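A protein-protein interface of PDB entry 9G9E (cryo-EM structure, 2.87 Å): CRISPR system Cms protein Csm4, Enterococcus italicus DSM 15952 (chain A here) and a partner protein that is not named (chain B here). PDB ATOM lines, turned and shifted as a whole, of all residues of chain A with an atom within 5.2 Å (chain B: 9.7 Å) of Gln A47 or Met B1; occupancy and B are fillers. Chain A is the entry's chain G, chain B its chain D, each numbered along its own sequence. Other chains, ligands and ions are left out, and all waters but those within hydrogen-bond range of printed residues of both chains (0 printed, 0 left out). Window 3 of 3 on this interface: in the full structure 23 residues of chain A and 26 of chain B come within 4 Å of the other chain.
CB of Tyr B2 touches O of Gln A46 (3.2 Å).
Tyr B2 touches Gln A47.
Gln A47 touches Val B203 (NE2 to CG1, 3.7 Å).
O of Lys B4 is in hydrogen-bond range of N of Val B202 (2.9 Å).
The side-chain amide nitrogen (ND2) of Asn B155 lies close to the side-chain hydroxyl (OH) of Tyr B2 (3.4 Å).
The backbone carbonyl oxygen (O) of Glu A43 sits close to the side-chain amide oxygen (OE1) of Gln A47, at 3.1 Å.
O of Val B203 lies within hydrogen-bond range of N of Lys B4 (2.9 Å).
The side-chain carboxylate (OD1) of Asp B205 sits at hydrogen-bond distance from the backbone NH (N) of Met B1 (3.4 Å).
The side-chain amide oxygen of Gln A46 sits close to the side-chain carboxylate of Glu A43, 3.1 Å away.
Of the printed residues of chain B, Glu A43 touches Lys B4 (2.9 Å).
Leu A45 touches none of the printed residues of chain B.
Printed residues of chain B within 4 Å of Gln A46: Tyr B2 (3.2 Å).
No residue of chain B comes within 4 Å of Gln A48.
Leu A179 touches none of the printed residues of chain B.
Of the printed residues of chain B, Ala A182 touches Lys B4.
Of the printed residues of chain A, Tyr B2 touches Gln A46 (3.2 Å) and Gln A47 (3.6 Å).
Printed residues of chain A within 4 Å of Val B203: Gln A47 (3.7 Å).
The nearest residue of chain A that does not touch Met B1 is Gln A48 (4.1 Å).
The nearest printed residue of chain B that does not touch Ala A182 is Val B203 (4.5 Å).
The side-chain amino group (NZ) of Lys B4 is in salt-bridge range of the side-chain carboxylate (OE2) of Glu A43 (2.9 Å).
NZ of Lys B4 is in hydrogen-bond range of O of Ala A182, 3.0 Å away.
O of Gln A47 lies close to SD of Met B1 (3.2 Å).
Hydrophobic or aromatic side chains of chain B that line the printed part of chain A: Met B1, Tyr B2 and Val B203.
Hydrophobic or aromatic side chains of chain A that line the printed part of chain B: Ala A182.
Along chain A the printed residues that touch a printed residue of chain B span positions 43 to 182.
Among the printed residues, Asp or Glu carboxylates within 4 Å of a Lys or Arg side-chain nitrogen of the other chain: Glu A43 with Lys B4 (2.9 Å).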
ATOM      1  N   ILE A  42       2.839  25.161  39.148  1.00  0.00           N
ATOM      2  CA  ILE A  42       2.553  25.560  37.773  1.00  0.00           C
ATOM      3  C   ILE A  42       3.559  24.931  36.818  1.00  0.00           C
ATOM      4  O   ILE A  42       3.198  24.455  35.734  1.00  0.00           O
ATOM      5  CB  ILE A  42       2.540  27.096  37.657  1.00  0.00           C
ATOM      6  CG1 ILE A  42       1.306  27.673  38.354  1.00  0.00           C
ATOM      7  CG2 ILE A  42       2.578  27.528  36.201  1.00  0.00           C
ATOM      8  CD1 ILE A  42       1.268  29.182  38.378  1.00  0.00           C
ATOM      9  N   GLU A  43       4.836  24.914  37.207  1.00  0.00           N
ATOM     10  CA  GLU A  43       5.863  24.295  36.375  1.00  0.00           C
ATOM     11  C   GLU A  43       5.627  22.799  36.217  1.00  0.00           C
ATOM     12  O   GLU A  43       5.797  22.248  35.123  1.00  0.00           O
ATOM     13  CB  GLU A  43       7.244  24.556  36.973  1.00  0.00           C
ATOM     14  CG  GLU A  43       8.333  24.654  35.937  1.00  0.00           C
ATOM     15  CD  GLU A  43       8.114  25.819  35.001  1.00  0.00           C
ATOM     16  OE1 GLU A  43       7.653  26.878  35.472  1.00  0.00           O
ATOM     17  OE2 GLU A  43       8.388  25.670  33.793  1.00  0.00           O
ATOM     18  N   ALA A  44       5.248  22.121  37.302  1.00  0.00           N
ATOM     19  CA  ALA A  44       4.983  20.688  37.226  1.00  0.00           C
ATOM     20  C   ALA A  44       3.796  20.400  36.320  1.00  0.00           C
ATOM     21  O   ALA A  44       3.802  19.420  35.567  1.00  0.00           O
ATOM     22  CB  ALA A  44       4.745  20.122  38.626  1.00  0.00           C
ATOM     23  N   LEU A  45       2.761  21.239  36.385  1.00  0.00           N
ATOM     24  CA  LEU A  45       1.620  21.074  35.489  1.00  0.00           C
ATOM     25  C   LEU A  45       2.015  21.332  34.040  1.00  0.00           C
ATOM     26  O   LEU A  45       1.527  20.655  33.128  1.00  0.00           O
ATOM     27  CB  LEU A  45       0.484  22.001  35.913  1.00  0.00           C
ATOM     28  CG  LEU A  45      -0.167  21.656  37.250  1.00  0.00           C
ATOM     29  CD1 LEU A  45      -0.646  22.917  37.942  1.00  0.00           C
ATOM     30  CD2 LEU A  45      -1.315  20.682  37.052  1.00  0.00           C
ATOM     31  N   GLN A  46       2.889  22.315  33.808  1.00  0.00           N
ATOM     32  CA  GLN A  46       3.371  22.582  32.456  1.00  0.00           C
ATOM     33  C   GLN A  46       4.132  21.384  31.901  1.00  0.00           C
ATOM     34  O   GLN A  46       3.950  20.998  30.741  1.00  0.00           O
ATOM     35  CB  GLN A  46       4.254  23.829  32.452  1.00  0.00           C
ATOM     36  CG  GLN A  46       3.489  25.139  32.487  1.00  0.00           C
ATOM     37  CD  GLN A  46       4.404  26.347  32.444  1.00  0.00           C
ATOM     38  OE1 GLN A  46       5.625  26.212  32.382  1.00  0.00           O
ATOM     39  NE2 GLN A  46       3.816  27.537  32.479  1.00  0.00           N
ATOM     40  N   GLN A  47       4.988  20.779  32.723  1.00  0.00           N
ATOM     41  CA  GLN A  47       5.799  19.644  32.304  1.00  0.00           C
ATOM     42  C   GLN A  47       5.093  18.308  32.484  1.00  0.00           C
ATOM     43  O   GLN A  47       5.713  17.266  32.247  1.00  0.00           O
ATOM     44  CB  GLN A  47       7.123  19.637  33.072  1.00  0.00           C
ATOM     45  CG  GLN A  47       8.305  20.160  32.277  1.00  0.00           C
ATOM     46  CD  GLN A  47       8.449  21.664  32.373  1.00  0.00           C
ATOM     47  OE1 GLN A  47       8.397  22.235  33.462  1.00  0.00           O
ATOM     48  NE2 GLN A  47       8.631  22.316  31.231  1.00  0.00           N
ATOM     49  N   GLN A  48       3.827  18.315  32.904  1.00  0.00           N
ATOM     50  CA  GLN A  48       3.020  17.101  33.035  1.00  0.00           C
ATOM     51  C   GLN A  48       3.668  16.086  33.976  1.00  0.00           C
ATOM     52  O   GLN A  48       3.660  14.880  33.719  1.00  0.00           O
ATOM     53  CB  GLN A  48       2.747  16.473  31.666  1.00  0.00           C
ATOM     54  CG  GLN A  48       1.482  16.978  30.994  1.00  0.00           C
ATOM     55  CD  GLN A  48       1.658  17.177  29.502  1.00  0.00           C
ATOM     56  OE1 GLN A  48       2.080  18.242  29.052  1.00  0.00           O
ATOM     57  NE2 GLN A  48       1.335  16.148  28.726  1.00  0.00           N
ATOM     58  N   LEU A  49       4.234  16.574  35.075  1.00  0.00           N
ATOM     59  CA  LEU A  49       4.796  15.705  36.095  1.00  0.00           C
ATOM     60  C   LEU A  49       3.777  15.452  37.204  1.00  0.00           C
ATOM     61  O   LEU A  49       2.735  16.105  37.291  1.00  0.00           O
ATOM     62  CB  LEU A  49       6.074  16.306  36.680  1.00  0.00           C
ATOM     63  CG  LEU A  49       7.296  16.405  35.769  1.00  0.00           C
ATOM     64  CD1 LEU A  49       8.012  17.728  35.983  1.00  0.00           C
ATOM     65  CD2 LEU A  49       8.239  15.236  36.012  1.00  0.00           C
ATOM     66  N   LEU A 179      12.276  20.942  38.010  1.00  0.00           N
ATOM     67  CA  LEU A 179      11.338  22.056  38.112  1.00  0.00           C
ATOM     68  C   LEU A 179      12.065  23.392  38.187  1.00  0.00           C
ATOM     69  O   LEU A 179      11.637  24.368  37.568  1.00  0.00           O
ATOM     70  CB  LEU A 179      10.427  21.867  39.325  1.00  0.00           C
ATOM     71  CG  LEU A 179       9.404  20.739  39.197  1.00  0.00           C
ATOM     72  CD1 LEU A 179       8.547  20.645  40.446  1.00  0.00           C
ATOM     73  CD2 LEU A 179       8.544  20.942  37.963  1.00  0.00           C
ATOM     74  N   ALA A 182      13.436  24.333  34.741  1.00  0.00           N
ATOM     75  CA  ALA A 182      12.406  24.954  33.911  1.00  0.00           C
ATOM     76  C   ALA A 182      12.007  26.332  34.439  1.00  0.00           C
ATOM     77  O   ALA A 182      11.660  27.225  33.654  1.00  0.00           O
ATOM     78  CB  ALA A 182      11.186  24.040  33.818  1.00  0.00           C
ATOM     79  N   MET B   1       7.054  16.995  25.447  1.00  0.00           N
ATOM     80  CA  MET B   1       6.049  17.510  26.369  1.00  0.00           C
ATOM     81  C   MET B   1       5.959  19.029  26.273  1.00  0.00           C
ATOM     82  O   MET B   1       5.325  19.564  25.363  1.00  0.00           O
ATOM     83  CB  MET B   1       6.370  17.081  27.803  1.00  0.00           C
ATOM     84  CG  MET B   1       5.724  15.764  28.209  1.00  0.00           C
ATOM     85  SD  MET B   1       6.181  15.219  29.867  1.00  0.00           S
ATOM     86  CE  MET B   1       7.797  15.970  30.047  1.00  0.00           C
ATOM     87  N   TYR B   2       6.593  19.722  27.213  1.00  0.00           N
ATOM     88  CA  TYR B   2       6.640  21.176  27.216  1.00  0.00           C
ATOM     89  C   TYR B   2       8.041  21.646  26.851  1.00  0.00           C
ATOM     90  O   TYR B   2       9.035  21.119  27.357  1.00  0.00           O
ATOM     91  CB  TYR B   2       6.237  21.739  28.579  1.00  0.00           C
ATOM     92  CG  TYR B   2       5.821  23.191  28.535  1.00  0.00           C
ATOM     93  CD1 TYR B   2       4.509  23.547  28.255  1.00  0.00           C
ATOM     94  CD2 TYR B   2       6.739  24.205  28.772  1.00  0.00           C
ATOM     95  CE1 TYR B   2       4.122  24.871  28.212  1.00  0.00           C
ATOM     96  CE2 TYR B   2       6.360  25.533  28.732  1.00  0.00           C
ATOM     97  CZ  TYR B   2       5.052  25.860  28.451  1.00  0.00           C
ATOM     98  OH  TYR B   2       4.669  27.179  28.411  1.00  0.00           O
ATOM     99  N   SER B   3       8.114  22.640  25.970  1.00  0.00           N
ATOM    100  CA  SER B   3       9.383  23.114  25.442  1.00  0.00           C
ATOM    101  C   SER B   3       9.479  24.628  25.566  1.00  0.00           C
ATOM    102  O   SER B   3       8.472  25.340  25.543  1.00  0.00           O
ATOM    103  CB  SER B   3       9.566  22.704  23.975  1.00  0.00           C
ATOM    104  OG  SER B   3       9.404  21.306  23.812  1.00  0.00           O
ATOM    105  N   LYS B   4      10.711  25.106  25.703  1.00  0.00           N
ATOM    106  CA  LYS B   4      11.011  26.528  25.699  1.00  0.00           C
ATOM    107  C   LYS B   4      12.247  26.744  24.843  1.00  0.00           C
ATOM    108  O   LYS B   4      13.274  26.093  25.062  1.00  0.00           O
ATOM    109  CB  LYS B   4      11.251  27.053  27.116  1.00  0.00           C
ATOM    110  CG  LYS B   4       9.998  27.513  27.824  1.00  0.00           C
ATOM    111  CD  LYS B   4      10.275  27.714  29.298  1.00  0.00           C
ATOM    112  CE  LYS B   4      10.005  26.434  30.062  1.00  0.00           C
ATOM    113  NZ  LYS B   4       9.724  26.690  31.491  1.00  0.00           N
ATOM    114  N   ASN B 155       7.533  29.893  24.485  1.00  0.00           N
ATOM    115  CA  ASN B 155       6.943  28.743  25.157  1.00  0.00           C
ATOM    116  C   ASN B 155       6.107  27.950  24.160  1.00  0.00           C
ATOM    117  O   ASN B 155       5.180  28.496  23.553  1.00  0.00           O
ATOM    118  CB  ASN B 155       6.078  29.199  26.330  1.00  0.00           C
ATOM    119  CG  ASN B 155       6.849  30.015  27.344  1.00  0.00           C
ATOM    120  OD1 ASN B 155       6.993  31.228  27.198  1.00  0.00           O
ATOM    121  ND2 ASN B 155       7.332  29.357  28.388  1.00  0.00           N
ATOM    122  N   VAL B 156       6.426  26.668  23.992  1.00  0.00           N
ATOM    123  CA  VAL B 156       5.669  25.810  23.092  1.00  0.00           C
ATOM    124  C   VAL B 156       4.511  25.195  23.864  1.00  0.00           C
ATOM    125  O   VAL B 156       4.610  24.075  24.376  1.00  0.00           O
ATOM    126  CB  VAL B 156       6.566  24.722  22.470  1.00  0.00           C
ATOM    127  CG1 VAL B 156       5.774  23.870  21.490  1.00  0.00           C
ATOM    128  CG2 VAL B 156       7.756  25.355  21.783  1.00  0.00           C
ATOM    129  N   GLU B 157       3.408  25.937  23.969  1.00  0.00           N
ATOM    130  CA  GLU B 157       2.204  25.392  24.579  1.00  0.00           C
ATOM    131  C   GLU B 157       1.476  24.452  23.628  1.00  0.00           C
ATOM    132  O   GLU B 157       0.803  23.519  24.079  1.00  0.00           O
ATOM    133  CB  GLU B 157       1.287  26.529  25.031  1.00  0.00           C
ATOM    134  CG  GLU B 157       2.024  27.840  25.255  1.00  0.00           C
ATOM    135  CD  GLU B 157       1.266  28.799  26.150  1.00  0.00           C
ATOM    136  OE1 GLU B 157       1.921  29.567  26.885  1.00  0.00           O
ATOM    137  OE2 GLU B 157       0.017  28.784  26.122  1.00  0.00           O
ATOM    138  N   ASN B 158       1.592  24.689  22.323  1.00  0.00           N
ATOM    139  CA  ASN B 158       1.102  23.771  21.303  1.00  0.00           C
ATOM    140  C   ASN B 158       2.199  23.567  20.272  1.00  0.00           C
ATOM    141  O   ASN B 158       2.853  24.530  19.858  1.00  0.00           O
ATOM    142  CB  ASN B 158      -0.172  24.299  20.634  1.00  0.00           C
ATOM    143  CG  ASN B 158      -0.628  23.420  19.489  1.00  0.00           C
ATOM    144  OD1 ASN B 158      -0.866  23.897  18.381  1.00  0.00           O
ATOM    145  ND2 ASN B 158      -0.754  22.123  19.753  1.00  0.00           N
ATOM    146  N   ILE B 159       2.400  22.314  19.861  1.00  0.00           N
ATOM    147  CA  ILE B 159       3.500  21.997  18.955  1.00  0.00           C
ATOM    148  C   ILE B 159       3.114  22.279  17.504  1.00  0.00           C
ATOM    149  O   ILE B 159       3.985  22.526  16.663  1.00  0.00           O
ATOM    150  CB  ILE B 159       3.969  20.535  19.130  1.00  0.00           C
ATOM    151  CG1 ILE B 159       4.217  20.152  20.601  1.00  0.00           C
ATOM    152  CG2 ILE B 159       5.235  20.269  18.329  1.00  0.00           C
ATOM    153  CD1 ILE B 159       2.984  19.876  21.463  1.00  0.00           C
ATOM    154  N   ASN B 160       1.821  22.262  17.184  1.00  0.00           N
ATOM    155  CA  ASN B 160       1.390  22.425  15.801  1.00  0.00           C
ATOM    156  C   ASN B 160       1.473  23.865  15.311  1.00  0.00           C
ATOM    157  O   ASN B 160       1.538  24.086  14.097  1.00  0.00           O
ATOM    158  CB  ASN B 160      -0.040  21.908  15.636  1.00  0.00           C
ATOM    159  CG  ASN B 160      -0.196  20.478  16.108  1.00  0.00           C
ATOM    160  OD1 ASN B 160       0.757  19.700  16.091  1.00  0.00           O
ATOM    161  ND2 ASN B 160      -1.402  20.124  16.536  1.00  0.00           N
ATOM    162  N   VAL B 162       3.933  26.074  16.160  1.00  0.00           N
ATOM    163  CA  VAL B 162       5.271  26.639  16.312  1.00  0.00           C
ATOM    164  C   VAL B 162       5.716  27.321  15.023  1.00  0.00           C
ATOM    165  O   VAL B 162       6.291  28.414  15.049  1.00  0.00           O
ATOM    166  CB  VAL B 162       6.271  25.556  16.753  1.00  0.00           C
ATOM    167  CG1 VAL B 162       7.617  26.184  17.071  1.00  0.00           C
ATOM    168  CG2 VAL B 162       5.739  24.817  17.965  1.00  0.00           C
ATOM    169  N   THR B 201      16.741  25.267  21.735  1.00  0.00           N
ATOM    170  CA  THR B 201      15.708  24.792  22.650  1.00  0.00           C
ATOM    171  C   THR B 201      16.332  24.504  24.009  1.00  0.00           C
ATOM    172  O   THR B 201      17.071  23.527  24.167  1.00  0.00           O
ATOM    173  CB  THR B 201      15.036  23.546  22.082  1.00  0.00           C
ATOM    174  OG1 THR B 201      14.333  23.886  20.881  1.00  0.00           O
ATOM    175  CG2 THR B 201      14.057  22.967  23.081  1.00  0.00           C
ATOM    176  N   VAL B 202      16.043  25.353  24.992  1.00  0.00           N
ATOM    177  CA  VAL B 202      16.606  25.163  26.323  1.00  0.00           C
ATOM    178  C   VAL B 202      15.772  24.207  27.171  1.00  0.00           C
ATOM    179  O   VAL B 202      16.316  23.541  28.058  1.00  0.00           O
ATOM    180  CB  VAL B 202      16.786  26.513  27.037  1.00  0.00           C
ATOM    181  CG1 VAL B 202      17.988  27.246  26.474  1.00  0.00           C
ATOM    182  CG2 VAL B 202      15.532  27.358  26.912  1.00  0.00           C
ATOM    183  N   VAL B 203      14.464  24.118  26.932  1.00  0.00           N
ATOM    184  CA  VAL B 203      13.597  23.227  27.696  1.00  0.00           C
ATOM    185  C   VAL B 203      12.855  22.311  26.735  1.00  0.00           C
ATOM    186  O   VAL B 203      12.355  22.756  25.698  1.00  0.00           O
ATOM    187  CB  VAL B 203      12.602  24.010  28.579  1.00  0.00           C
ATOM    188  CG1 VAL B 203      11.859  23.065  29.510  1.00  0.00           C
ATOM    189  CG2 VAL B 203      13.327  25.073  29.381  1.00  0.00           C
ATOM    190  N   GLY B 204      12.793  21.031  27.077  1.00  0.00           N
ATOM    191  CA  GLY B 204      12.036  20.084  26.286  1.00  0.00           C
ATOM    192  C   GLY B 204      12.854  19.423  25.196  1.00  0.00           C
ATOM    193  O   GLY B 204      14.084  19.517  25.130  1.00  0.00           O
ATOM    194  N   ASP B 205      12.132  18.732  24.316  1.00  0.00           N
ATOM    195  CA  ASP B 205      12.733  17.956  23.242  1.00  0.00           C
ATOM    196  C   ASP B 205      12.446  18.521  21.857  1.00  0.00           C
ATOM    197  O   ASP B 205      12.822  17.894  20.860  1.00  0.00           O
ATOM    198  CB  ASP B 205      12.256  16.498  23.304  1.00  0.00           C
ATOM    199  CG  ASP B 205      10.751  16.359  23.127  1.00  0.00           C
ATOM    200  OD1 ASP B 205       9.988  17.108  23.774  1.00  0.00           O
ATOM    201  OD2 ASP B 205      10.328  15.495  22.331  1.00  0.00           O
ATOM    202  N   PHE B 206      11.789  19.675  21.764  1.00  0.00           N
ATOM    203  CA  PHE B 206      11.454  20.237  20.462  1.00  0.00           C
ATOM    204  C   PHE B 206      12.717  20.613  19.697  1.00  0.00           C
ATOM    205  O   PHE B 206      13.680  21.132  20.268  1.00  0.00           O
ATOM    206  CB  PHE B 206      10.554  21.462  20.626  1.00  0.00           C
ATOM    207  CG  PHE B 206       9.994  21.978  19.332  1.00  0.00           C
ATOM    208  CD1 PHE B 206       8.879  21.388  18.763  1.00  0.00           C
ATOM    209  CD2 PHE B 206      10.584  23.049  18.682  1.00  0.00           C
ATOM    210  CE1 PHE B 206       8.361  21.855  17.573  1.00  0.00           C
ATOM    211  CE2 PHE B 206      10.070  23.521  17.491  1.00  0.00           C
ATOM    212  CZ  PHE B 206       8.957  22.922  16.936  1.00  0.00           C
ATOM    213  N   ASP B 207      12.707  20.345  18.393  1.00  0.00           N
ATOM    214  CA  ASP B 207      13.851  20.615  17.528  1.00  0.00           C
ATOM    215  C   ASP B 207      13.677  21.992  16.898  1.00  0.00           C
ATOM    216  O   ASP B 207      12.851  22.172  15.997  1.00  0.00           O
ATOM    217  CB  ASP B 207      13.982  19.532  16.460  1.00  0.00           C
ATOM    218  CG  ASP B 207      15.296  19.610  15.708  1.00  0.00           C
ATOM    219  OD1 ASP B 207      16.343  19.285  16.305  1.00  0.00           O
ATOM    220  OD2 ASP B 207      15.280  19.995  14.520  1.00  0.00           O
